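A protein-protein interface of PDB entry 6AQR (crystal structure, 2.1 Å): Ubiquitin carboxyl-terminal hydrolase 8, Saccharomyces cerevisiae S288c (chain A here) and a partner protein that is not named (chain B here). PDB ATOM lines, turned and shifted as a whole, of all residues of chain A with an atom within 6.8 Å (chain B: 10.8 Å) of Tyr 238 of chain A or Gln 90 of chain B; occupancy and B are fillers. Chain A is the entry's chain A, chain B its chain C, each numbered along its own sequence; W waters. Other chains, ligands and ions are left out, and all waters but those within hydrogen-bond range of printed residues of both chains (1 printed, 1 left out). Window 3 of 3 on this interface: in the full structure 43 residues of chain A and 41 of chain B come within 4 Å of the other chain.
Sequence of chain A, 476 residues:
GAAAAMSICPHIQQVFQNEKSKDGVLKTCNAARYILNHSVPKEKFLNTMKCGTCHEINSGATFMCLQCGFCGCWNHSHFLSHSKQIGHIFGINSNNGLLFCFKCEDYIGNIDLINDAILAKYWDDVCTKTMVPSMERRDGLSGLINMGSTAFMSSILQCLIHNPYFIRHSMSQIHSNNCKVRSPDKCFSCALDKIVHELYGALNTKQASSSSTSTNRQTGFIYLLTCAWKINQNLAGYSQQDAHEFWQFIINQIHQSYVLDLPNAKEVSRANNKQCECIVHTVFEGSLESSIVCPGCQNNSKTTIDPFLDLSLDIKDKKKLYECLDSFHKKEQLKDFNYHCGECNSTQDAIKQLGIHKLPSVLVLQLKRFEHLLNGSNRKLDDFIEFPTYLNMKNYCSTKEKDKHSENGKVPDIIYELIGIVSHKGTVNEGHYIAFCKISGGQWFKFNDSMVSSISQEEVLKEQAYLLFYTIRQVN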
ATOM      1  N   MET A 147       1.676 -24.189  26.642  1.00  0.00           N
ATOM      2  CA  MET A 147       2.511 -25.387  26.422  1.00  0.00           C
ATOM      3  C   MET A 147       3.580 -25.564  27.493  1.00  0.00           C
ATOM      4  O   MET A 147       4.376 -26.519  27.439  1.00  0.00           O
ATOM      5  CB  MET A 147       3.146 -25.420  25.028  1.00  0.00           C
ATOM      6  CG  MET A 147       2.171 -25.249  23.890  1.00  0.00           C
ATOM      7  SD  MET A 147       0.866 -26.474  23.902  1.00  0.00           S
ATOM      8  CE  MET A 147      -0.011 -26.016  22.390  1.00  0.00           C
ATOM      9  N   GLY A 148       3.566 -24.669  28.482  1.00  0.00           N
ATOM     10  CA  GLY A 148       4.508 -24.760  29.617  1.00  0.00           C
ATOM     11  C   GLY A 148       4.615 -23.368  30.202  1.00  0.00           C
ATOM     12  O   GLY A 148       3.958 -23.062  31.158  1.00  0.00           O
ATOM     13  N   SER A 149       5.427 -22.502  29.599  1.00  0.00           N
ATOM     14  CA  SER A 149       5.430 -21.083  29.988  1.00  0.00           C
ATOM     15  C   SER A 149       5.241 -20.228  28.743  1.00  0.00           C
ATOM     16  O   SER A 149       5.908 -19.235  28.617  1.00  0.00           O
ATOM     17  CB  SER A 149       6.760 -20.719  30.673  1.00  0.00           C
ATOM     18  OG  SER A 149       6.902 -21.486  31.843  1.00  0.00           O
ATOM     19  N   THR A 150       4.316 -20.606  27.848  1.00  0.00           N
ATOM     20  CA  THR A 150       4.157 -19.871  26.580  1.00  0.00           C
ATOM     21  C   THR A 150       3.302 -18.564  26.632  1.00  0.00           C
ATOM     22  O   THR A 150       3.105 -17.937  25.603  1.00  0.00           O
ATOM     23  CB  THR A 150       3.663 -20.839  25.514  1.00  0.00           C
ATOM     24  OG1 THR A 150       2.419 -21.425  25.960  1.00  0.00           O
ATOM     25  CG2 THR A 150       4.680 -21.906  25.401  1.00  0.00           C
ATOM     26  N   PHE A 152       4.132 -15.567  27.373  1.00  0.00           N
ATOM     27  CA  PHE A 152       4.897 -14.449  26.817  1.00  0.00           C
ATOM     28  C   PHE A 152       4.941 -14.572  25.284  1.00  0.00           C
ATOM     29  O   PHE A 152       5.221 -13.589  24.588  1.00  0.00           O
ATOM     30  CB  PHE A 152       6.344 -14.373  27.412  1.00  0.00           C
ATOM     31  CG  PHE A 152       7.295 -15.450  26.894  1.00  0.00           C
ATOM     32  CD1 PHE A 152       8.049 -15.230  25.725  1.00  0.00           C
ATOM     33  CD2 PHE A 152       7.412 -16.702  27.580  1.00  0.00           C
ATOM     34  CE1 PHE A 152       8.933 -16.209  25.246  1.00  0.00           C
ATOM     35  CE2 PHE A 152       8.268 -17.715  27.104  1.00  0.00           C
ATOM     36  CZ  PHE A 152       9.042 -17.482  25.932  1.00  0.00           C
ATOM     37  N   MET A 153       4.705 -15.781  24.764  1.00  0.00           N
ATOM     38  CA  MET A 153       4.662 -15.954  23.340  1.00  0.00           C
ATOM     39  C   MET A 153       3.286 -15.658  22.804  1.00  0.00           C
ATOM     40  O   MET A 153       3.144 -15.007  21.805  1.00  0.00           O
ATOM     41  CB  MET A 153       5.087 -17.391  22.934  1.00  0.00           C
ATOM     42  CG  MET A 153       6.487 -17.692  23.561  1.00  0.00           C
ATOM     43  SD  MET A 153       6.928 -19.442  23.315  1.00  0.00           S
ATOM     44  CE  MET A 153       7.286 -19.302  21.530  1.00  0.00           C
ATOM     45  N   TRP A 229      12.672 -22.985  18.953  1.00  0.00           N
ATOM     46  CA  TRP A 229      13.625 -23.839  19.663  1.00  0.00           C
ATOM     47  C   TRP A 229      14.915 -23.983  18.850  1.00  0.00           C
ATOM     48  O   TRP A 229      15.978 -23.980  19.427  1.00  0.00           O
ATOM     49  CB  TRP A 229      13.045 -25.235  19.985  1.00  0.00           C
ATOM     50  CG  TRP A 229      14.029 -26.149  20.660  1.00  0.00           C
ATOM     51  CD1 TRP A 229      14.247 -26.287  22.028  1.00  0.00           C
ATOM     52  CD2 TRP A 229      14.953 -27.020  20.011  1.00  0.00           C
ATOM     53  NE1 TRP A 229      15.258 -27.188  22.237  1.00  0.00           N
ATOM     54  CE2 TRP A 229      15.692 -27.671  21.023  1.00  0.00           C
ATOM     55  CE3 TRP A 229      15.240 -27.301  18.672  1.00  0.00           C
ATOM     56  CZ2 TRP A 229      16.694 -28.605  20.736  1.00  0.00           C
ATOM     57  CZ3 TRP A 229      16.286 -28.231  18.367  1.00  0.00           C
ATOM     58  CH2 TRP A 229      16.972 -28.882  19.410  1.00  0.00           C
ATOM     59  N   GLN A 233      16.604 -21.487  22.307  1.00  0.00           N
ATOM     60  CA  GLN A 233      15.884 -22.365  23.179  1.00  0.00           C
ATOM     61  C   GLN A 233      15.257 -21.605  24.338  1.00  0.00           C
ATOM     62  O   GLN A 233      14.128 -21.914  24.774  1.00  0.00           O
ATOM     63  CB  GLN A 233      16.797 -23.472  23.694  1.00  0.00           C
ATOM     64  CG  GLN A 233      17.526 -24.199  22.588  1.00  0.00           C
ATOM     65  CD  GLN A 233      18.352 -25.373  23.104  1.00  0.00           C
ATOM     66  OE1 GLN A 233      18.812 -26.217  22.325  1.00  0.00           O
ATOM     67  NE2 GLN A 233      18.522 -25.439  24.407  1.00  0.00           N
ATOM     68  N   ASN A 234      15.958 -20.598  24.820  1.00  0.00           N
ATOM     69  CA  ASN A 234      15.417 -19.783  25.929  1.00  0.00           C
ATOM     70  C   ASN A 234      14.076 -19.089  25.652  1.00  0.00           C
ATOM     71  O   ASN A 234      13.302 -18.850  26.611  1.00  0.00           O
ATOM     72  CB  ASN A 234      16.422 -18.704  26.331  1.00  0.00           C
ATOM     73  CG  ASN A 234      17.632 -19.289  27.021  1.00  0.00           C
ATOM     74  OD1 ASN A 234      17.584 -20.382  27.606  1.00  0.00           O
ATOM     75  ND2 ASN A 234      18.708 -18.554  26.993  1.00  0.00           N
ATOM     76  N   LEU A 235      13.827 -18.751  24.389  1.00  0.00           N
ATOM     77  CA  LEU A 235      12.560 -18.090  23.995  1.00  0.00           C
ATOM     78  C   LEU A 235      11.588 -19.053  23.350  1.00  0.00           C
ATOM     79  O   LEU A 235      10.686 -18.659  22.634  1.00  0.00           O
ATOM     80  CB  LEU A 235      12.842 -16.889  23.063  1.00  0.00           C
ATOM     81  CG  LEU A 235      13.726 -15.715  23.600  1.00  0.00           C
ATOM     82  CD1 LEU A 235      13.877 -14.568  22.593  1.00  0.00           C
ATOM     83  CD2 LEU A 235      13.164 -15.147  24.871  1.00  0.00           C
ATOM     84  N   ALA A 236      11.766 -20.336  23.600  1.00  0.00           N
ATOM     85  CA  ALA A 236      10.909 -21.324  22.964  1.00  0.00           C
ATOM     86  C   ALA A 236       9.758 -21.886  23.840  1.00  0.00           C
ATOM     87  O   ALA A 236       9.020 -22.752  23.405  1.00  0.00           O
ATOM     88  CB  ALA A 236      11.769 -22.429  22.349  1.00  0.00           C
ATOM     89  N   GLY A 237       9.621 -21.405  25.079  1.00  0.00           N
ATOM     90  CA  GLY A 237       8.373 -21.634  25.822  1.00  0.00           C
ATOM     91  C   GLY A 237       8.488 -22.527  27.041  1.00  0.00           C
ATOM     92  O   GLY A 237       7.521 -22.685  27.727  1.00  0.00           O
ATOM     93  N   TYR A 238       9.675 -23.084  27.311  1.00  0.00           N
ATOM     94  CA  TYR A 238       9.918 -23.853  28.525  1.00  0.00           C
ATOM     95  C   TYR A 238       9.945 -23.052  29.809  1.00  0.00           C
ATOM     96  O   TYR A 238       9.428 -23.465  30.812  1.00  0.00           O
ATOM     97  CB  TYR A 238      11.248 -24.623  28.350  1.00  0.00           C
ATOM     98  CG  TYR A 238      11.691 -25.351  29.584  1.00  0.00           C
ATOM     99  CD1 TYR A 238      10.972 -26.460  30.063  1.00  0.00           C
ATOM    100  CD2 TYR A 238      12.776 -24.877  30.344  1.00  0.00           C
ATOM    101  CE1 TYR A 238      11.343 -27.110  31.237  1.00  0.00           C
ATOM    102  CE2 TYR A 238      13.138 -25.520  31.523  1.00  0.00           C
ATOM    103  CZ  TYR A 238      12.415 -26.644  31.941  1.00  0.00           C
ATOM    104  OH  TYR A 238      12.736 -27.284  33.084  1.00  0.00           O
ATOM    105  N   SER A 239      10.576 -21.893  29.778  1.00  0.00           N
ATOM    106  CA  SER A 239      10.792 -21.045  30.957  1.00  0.00           C
ATOM    107  C   SER A 239      10.157 -19.687  30.776  1.00  0.00           C
ATOM    108  O   SER A 239       9.848 -19.277  29.653  1.00  0.00           O
ATOM    109  CB  SER A 239      12.287 -20.793  31.169  1.00  0.00           C
ATOM    110  OG  SER A 239      12.828 -20.288  29.943  1.00  0.00           O
ATOM    111  N   GLN A 240       9.973 -18.981  31.868  1.00  0.00           N
ATOM    112  CA  GLN A 240       9.329 -17.692  31.825  1.00  0.00           C
ATOM    113  C   GLN A 240      10.283 -16.636  31.222  1.00  0.00           C
ATOM    114  O   GLN A 240      11.465 -16.624  31.530  1.00  0.00           O
ATOM    115  CB  GLN A 240       8.835 -17.267  33.206  1.00  0.00           C
ATOM    116  CG  GLN A 240       7.771 -18.228  33.766  1.00  0.00           C
ATOM    117  CD  GLN A 240       6.774 -17.624  34.765  1.00  0.00           C
ATOM    118  OE1 GLN A 240       6.848 -16.465  35.162  1.00  0.00           O
ATOM    119  NE2 GLN A 240       5.809 -18.436  35.156  1.00  0.00           N
ATOM    120  N   CYS B  73       2.692 -35.439  19.331  1.00  0.00           N
ATOM    121  CA  CYS B  73       3.982 -34.867  18.844  1.00  0.00           C
ATOM    122  C   CYS B  73       4.305 -35.487  17.498  1.00  0.00           C
ATOM    123  O   CYS B  73       4.400 -36.720  17.412  1.00  0.00           O
ATOM    124  CB  CYS B  73       5.112 -35.187  19.796  1.00  0.00           C
ATOM    125  SG  CYS B  73       6.768 -34.571  19.311  1.00  0.00           S
ATOM    126  N   ASN B  75       7.023 -35.282  15.917  1.00  0.00           N
ATOM    127  CA  ASN B  75       8.449 -35.611  15.825  1.00  0.00           C
ATOM    128  C   ASN B  75       8.849 -37.017  16.333  1.00  0.00           C
ATOM    129  O   ASN B  75       9.814 -37.601  15.830  1.00  0.00           O
ATOM    130  CB  ASN B  75       9.308 -34.499  16.488  1.00  0.00           C
ATOM    131  CG  ASN B  75      10.764 -34.634  16.132  1.00  0.00           C
ATOM    132  OD1 ASN B  75      11.101 -34.489  14.973  1.00  0.00           O
ATOM    133  ND2 ASN B  75      11.602 -35.020  17.081  1.00  0.00           N
ATOM    134  N   CYS B  76       8.125 -37.528  17.339  1.00  0.00           N
ATOM    135  CA  CYS B  76       8.358 -38.833  17.904  1.00  0.00           C
ATOM    136  C   CYS B  76       7.115 -39.725  17.805  1.00  0.00           C
ATOM    137  O   CYS B  76       7.184 -40.884  18.228  1.00  0.00           O
ATOM    138  CB  CYS B  76       8.770 -38.725  19.346  1.00  0.00           C
ATOM    139  SG  CYS B  76       7.536 -37.948  20.405  1.00  0.00           S
ATOM    140  N   VAL B  80       1.601 -36.140  24.164  1.00  0.00           N
ATOM    141  CA  VAL B  80       2.336 -35.454  25.236  1.00  0.00           C
ATOM    142  C   VAL B  80       1.346 -34.608  25.929  1.00  0.00           C
ATOM    143  O   VAL B  80       0.539 -33.938  25.239  1.00  0.00           O
ATOM    144  CB  VAL B  80       3.449 -34.586  24.585  1.00  0.00           C
ATOM    145  CG1 VAL B  80       4.142 -33.687  25.598  1.00  0.00           C
ATOM    146  CG2 VAL B  80       4.462 -35.508  23.996  1.00  0.00           C
ATOM    147  N   ALA B  82      -0.334 -31.450  27.167  1.00  0.00           N
ATOM    148  CA  ALA B  82      -0.252 -30.172  26.479  1.00  0.00           C
ATOM    149  C   ALA B  82       0.585 -29.182  27.262  1.00  0.00           C
ATOM    150  O   ALA B  82       1.405 -28.455  26.645  1.00  0.00           O
ATOM    151  CB  ALA B  82      -1.640 -29.564  26.162  1.00  0.00           C
ATOM    152  N   ASN B  83       0.465 -29.184  28.596  1.00  0.00           N
ATOM    153  CA  ASN B  83       1.199 -28.201  29.379  1.00  0.00           C
ATOM    154  C   ASN B  83       2.685 -28.521  29.535  1.00  0.00           C
ATOM    155  O   ASN B  83       3.385 -27.834  30.225  1.00  0.00           O
ATOM    156  CB  ASN B  83       0.540 -27.961  30.729  1.00  0.00           C
ATOM    157  CG  ASN B  83       0.594 -29.202  31.643  1.00  0.00           C
ATOM    158  OD1 ASN B  83       0.853 -30.326  31.207  1.00  0.00           O
ATOM    159  ND2 ASN B  83       0.336 -28.986  32.924  1.00  0.00           N
ATOM    160  N   ARG B  84       3.153 -29.600  28.904  1.00  0.00           N
ATOM    161  CA  ARG B  84       4.548 -29.977  28.990  1.00  0.00           C
ATOM    162  C   ARG B  84       5.140 -30.082  27.597  1.00  0.00           C
ATOM    163  O   ARG B  84       6.283 -30.525  27.435  1.00  0.00           O
ATOM    164  CB  ARG B  84       4.732 -31.322  29.751  1.00  0.00           C
ATOM    165  CG  ARG B  84       4.598 -31.203  31.239  1.00  0.00           C
ATOM    166  CD  ARG B  84       5.871 -30.641  31.882  1.00  0.00           C
ATOM    167  NE  ARG B  84       7.016 -31.523  31.629  1.00  0.00           N
ATOM    168  CZ  ARG B  84       8.190 -31.412  32.248  1.00  0.00           C
ATOM    169  NH1 ARG B  84       8.381 -30.445  33.137  1.00  0.00           N
ATOM    170  NH2 ARG B  84       9.167 -32.275  31.965  1.00  0.00           N
ATOM    171  N   LEU B  85       4.359 -29.701  26.596  1.00  0.00           N
ATOM    172  CA  LEU B  85       4.852 -29.771  25.244  1.00  0.00           C
ATOM    173  C   LEU B  85       6.228 -29.005  25.081  1.00  0.00           C
ATOM    174  O   LEU B  85       7.114 -29.527  24.443  1.00  0.00           O
ATOM    175  CB  LEU B  85       3.840 -29.192  24.288  1.00  0.00           C
ATOM    176  CG  LEU B  85       4.317 -29.352  22.833  1.00  0.00           C
ATOM    177  CD1 LEU B  85       4.667 -30.783  22.476  1.00  0.00           C
ATOM    178  CD2 LEU B  85       3.278 -28.845  21.850  1.00  0.00           C
ATOM    179  N   ALA B  86       6.379 -27.806  25.646  1.00  0.00           N
ATOM    180  CA  ALA B  86       7.639 -27.066  25.386  1.00  0.00           C
ATOM    181  C   ALA B  86       8.775 -27.847  26.016  1.00  0.00           C
ATOM    182  O   ALA B  86       9.861 -27.960  25.444  1.00  0.00           O
ATOM    183  CB  ALA B  86       7.568 -25.638  25.943  1.00  0.00           C
ATOM    184  N   ALA B  87       8.538 -28.443  27.196  1.00  0.00           N
ATOM    185  CA  ALA B  87       9.616 -29.210  27.873  1.00  0.00           C
ATOM    186  C   ALA B  87       9.882 -30.491  27.093  1.00  0.00           C
ATOM    187  O   ALA B  87      11.027 -30.834  26.858  1.00  0.00           O
ATOM    188  CB  ALA B  87       9.265 -29.528  29.318  1.00  0.00           C
ATOM    189  N   HIS B  88       8.846 -31.161  26.609  1.00  0.00           N
ATOM    190  CA  HIS B  88       9.041 -32.331  25.750  1.00  0.00           C
ATOM    191  C   HIS B  88       9.962 -31.994  24.552  1.00  0.00           C
ATOM    192  O   HIS B  88      10.898 -32.723  24.270  1.00  0.00           O
ATOM    193  CB  HIS B  88       7.691 -32.901  25.228  1.00  0.00           C
ATOM    194  CG  HIS B  88       7.852 -34.013  24.229  1.00  0.00           C
ATOM    195  ND1 HIS B  88       8.158 -35.308  24.590  1.00  0.00           N
ATOM    196  CD2 HIS B  88       7.776 -34.019  22.874  1.00  0.00           C
ATOM    197  CE1 HIS B  88       8.289 -36.053  23.496  1.00  0.00           C
ATOM    198  NE2 HIS B  88       8.071 -35.299  22.442  1.00  0.00           N
ATOM    199  N   LEU B  89       9.636 -30.946  23.816  1.00  0.00           N
ATOM    200  CA  LEU B  89      10.339 -30.561  22.563  1.00  0.00           C
ATOM    201  C   LEU B  89      11.842 -30.300  22.802  1.00  0.00           C
ATOM    202  O   LEU B  89      12.679 -30.684  21.955  1.00  0.00           O
ATOM    203  CB  LEU B  89       9.694 -29.299  21.957  1.00  0.00           C
ATOM    204  CG  LEU B  89       8.353 -29.559  21.255  1.00  0.00           C
ATOM    205  CD1 LEU B  89       7.717 -28.257  20.763  1.00  0.00           C
ATOM    206  CD2 LEU B  89       8.506 -30.583  20.112  1.00  0.00           C
ATOM    207  N   GLN B  90      12.179 -29.753  23.974  1.00  0.00           N
ATOM    208  CA  GLN B  90      13.603 -29.595  24.382  1.00  0.00           C
ATOM    209  C   GLN B  90      14.438 -30.891  24.243  1.00  0.00           C
ATOM    210  O   GLN B  90      15.494 -30.860  23.600  1.00  0.00           O
ATOM    211  CB  GLN B  90      13.743 -29.035  25.782  1.00  0.00           C
ATOM    212  CG  GLN B  90      13.263 -27.607  25.865  1.00  0.00           C
ATOM    213  CD  GLN B  90      14.159 -26.745  26.732  1.00  0.00           C
ATOM    214  OE1 GLN B  90      14.574 -27.159  27.826  1.00  0.00           O
ATOM    215  NE2 GLN B  90      14.446 -25.526  26.257  1.00  0.00           N
ATOM    216  N   ARG B  91      13.924 -32.008  24.771  1.00  0.00           N
ATOM    217  CA  ARG B  91      14.535 -33.320  24.616  1.00  0.00           C
ATOM    218  C   ARG B  91      14.233 -33.920  23.268  1.00  0.00           C
ATOM    219  O   ARG B  91      15.091 -34.476  22.631  1.00  0.00           O
ATOM    220  CB  ARG B  91      14.120 -34.266  25.778  1.00  0.00           C
ATOM    221  CG  ARG B  91      14.567 -33.714  27.153  1.00  0.00           C
ATOM    222  CD  ARG B  91      14.082 -34.447  28.422  1.00  0.00           C
ATOM    223  NE  ARG B  91      12.623 -34.347  28.672  1.00  0.00           N
ATOM    224  CZ  ARG B  91      11.975 -33.308  29.219  1.00  0.00           C
ATOM    225  NH1 ARG B  91      12.602 -32.183  29.610  1.00  0.00           N
ATOM    226  NH2 ARG B  91      10.653 -33.393  29.376  1.00  0.00           N
ATOM    227  N   CYS B  92      13.022 -33.782  22.775  1.00  0.00           N
ATOM    228  CA  CYS B  92      12.650 -34.524  21.625  1.00  0.00           C
ATOM    229  C   CYS B  92      13.300 -33.998  20.350  1.00  0.00           C
ATOM    230  O   CYS B  92      13.610 -34.759  19.417  1.00  0.00           O
ATOM    231  CB  CYS B  92      11.118 -34.486  21.511  1.00  0.00           C
ATOM    232  SG  CYS B  92      10.499 -35.418  20.124  1.00  0.00           S
ATOM    233  N   LEU B  93      13.445 -32.679  20.263  1.00  0.00           N
ATOM    234  CA  LEU B  93      14.098 -32.078  19.091  1.00  0.00           C
ATOM    235  C   LEU B  93      15.604 -32.308  18.933  1.00  0.00           C
ATOM    236  O   LEU B  93      16.124 -32.103  17.855  1.00  0.00           O
ATOM    237  CB  LEU B  93      13.714 -30.584  18.967  1.00  0.00           C
ATOM    238  CG  LEU B  93      12.233 -30.341  18.535  1.00  0.00           C
ATOM    239  CD1 LEU B  93      11.802 -28.893  18.593  1.00  0.00           C
ATOM    240  CD2 LEU B  93      11.912 -30.935  17.167  1.00  0.00           C
ATOM    241  N   SER B  94      16.289 -32.734  19.988  1.00  0.00           N
ATOM    242  CA  SER B  94      17.718 -33.095  19.907  1.00  0.00           C
ATOM    243  C   SER B  94      18.095 -34.570  19.869  1.00  0.00           C
ATOM    244  O   SER B  94      17.485 -35.351  19.150  1.00  0.00           O
ATOM    245  CB  SER B  94      18.429 -32.457  21.045  1.00  0.00           C
ATOM    246  OG  SER B  94      17.635 -32.579  22.170  1.00  0.00           O
HETATM  247  O   HOH W   1       6.522 -27.279  28.868  1.00  0.00           O
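N of Leu 85 of chain B sits at hydrogen-bond distance from O of Met 147 of chain A (3.3 Å). O of Met 147 of chain A sits at hydrogen-bond distance from N of Ala 86 of chain B (3.0 Å). The backbone carbonyl oxygen (O) of Ala 82 of chain B sits close to the side-chain sulfur (SD) of Met 147 of chain A, 3.4 Å away. The backbone carbonyl oxygen (O) of Asn 83 of chain B sits close to the backbone carbonyl oxygen (O) of Met 147 of chain A (3.2 Å).
The backbone NH of Met 147 of chain A sits at hydrogen-bond distance from the side-chain hydroxyl of Thr 150 of chain A, 2.9 Å away. N of Ser 149 of chain A lies within hydrogen-bond range of O of Gly 237 of chain A (2.8 Å). The side-chain hydroxyl of Ser 149 of chain A lies within hydrogen-bond range of the backbone carbonyl oxygen of Tyr 238 of chain A (3.4 Å). The guanidinium group (NH1) of Arg 91 of chain B is in hydrogen-bond range of the backbone carbonyl oxygen (O) of Ala 87 of chain B (3.4 Å). The side-chain hydroxyl of Ser 94 of chain B is in hydrogen-bond range of the backbone carbonyl oxygen of Gln 90 of chain B (3.1 Å). The backbone carbonyl oxygen (O) of Arg 91 of chain B sits at hydrogen-bond distance from the side-chain hydroxyl (OG) of Ser 94 of chain B (3.2 Å).
Among the printed residues, pairs that only touch across the chains: Gly 148 of chain A with Asn 83 of chain B, Gly 237 of chain A with Ala 86 of chain B, Trp 229 of chain A with Leu 93 of chain B, Tyr 238 of chain A with Ala 86 of chain B, Tyr 238 of chain A with Ala 87 of chain B, Trp 229 of chain A with Gln 90 of chain B, Met 147 of chain A with Arg 84 of chain B, Tyr 238 of chain A with Gln 90 of chain B, Gln 233 of chain A with Gln 90 of chain B and Trp 229 of chain A with Ser 94 of chain B.
Printed residues of chain B within 4 Å of Gly 148 of chain A: Asn 83 (3.3 Å). No residue of chain B comes within 4 Å of Ser 149 of chain A. Met 153 of chain A touches none of the printed residues of chain B. Gln 233 of chain A touches one residue of chain B. No residue of chain B comes within 4 Å of Ala 236 of chain A. No residue of chain B comes within 4 Å of Ser 239 of chain A. Printed residues of chain A within 4 Å of Arg 84 of chain B: Met 147 (3.6 Å). Of the printed residues of chain A, Gln 90 of chain B touches Trp 229 (3.6 Å), Gln 233 (3.9 Å) and Tyr 238 (3.8 Å). Of the printed residues of chain A, Ser 94 of chain B touches Trp 229 (3.95 Å). The nearest residue of chain A that does not touch Gln 90 of chain B is Asn 234 of chain A (5.4 Å). The nearest printed residue of chain A that does not touch Leu 85 of chain B is Gly 148 of chain A (5.4 Å).
Of the 17 printed residues of chain B, 9 touch a printed residue of chain A. Hydrophobic or aromatic side chains of chain B within 4 Å of the printed part of chain A: Leu 85, Ala 86, Ala 87 and Leu 93. Of the 15 printed residues of chain A, 6 touch a printed residue of chain B. Hydrophobic or aromatic side chains of chain A that line the printed part of chain B: Met 147, Trp 229 and Tyr 238. Along chain A the printed residues that touch a printed residue of chain B span positions 147 to 238. Among the printed residues, 14 pairs touch across the chains. Among the printed residues, no Asp or Glu carboxylate lies within 4 Å of a Lys or Arg side-chain nitrogen of the other chain.
Water W1 lies within hydrogen-bond range of the backbone carbonyl oxygen (O) of Met 147 of chain A (2.7 Å), the backbone NH (N) of Ala 87 of chain B (2.9 Å), the backbone NH (N) of Ala 86 of chain B (3.3 Å) and the backbone carbonyl oxygen (O) of Asn 83 of chain B (3.5 Å).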
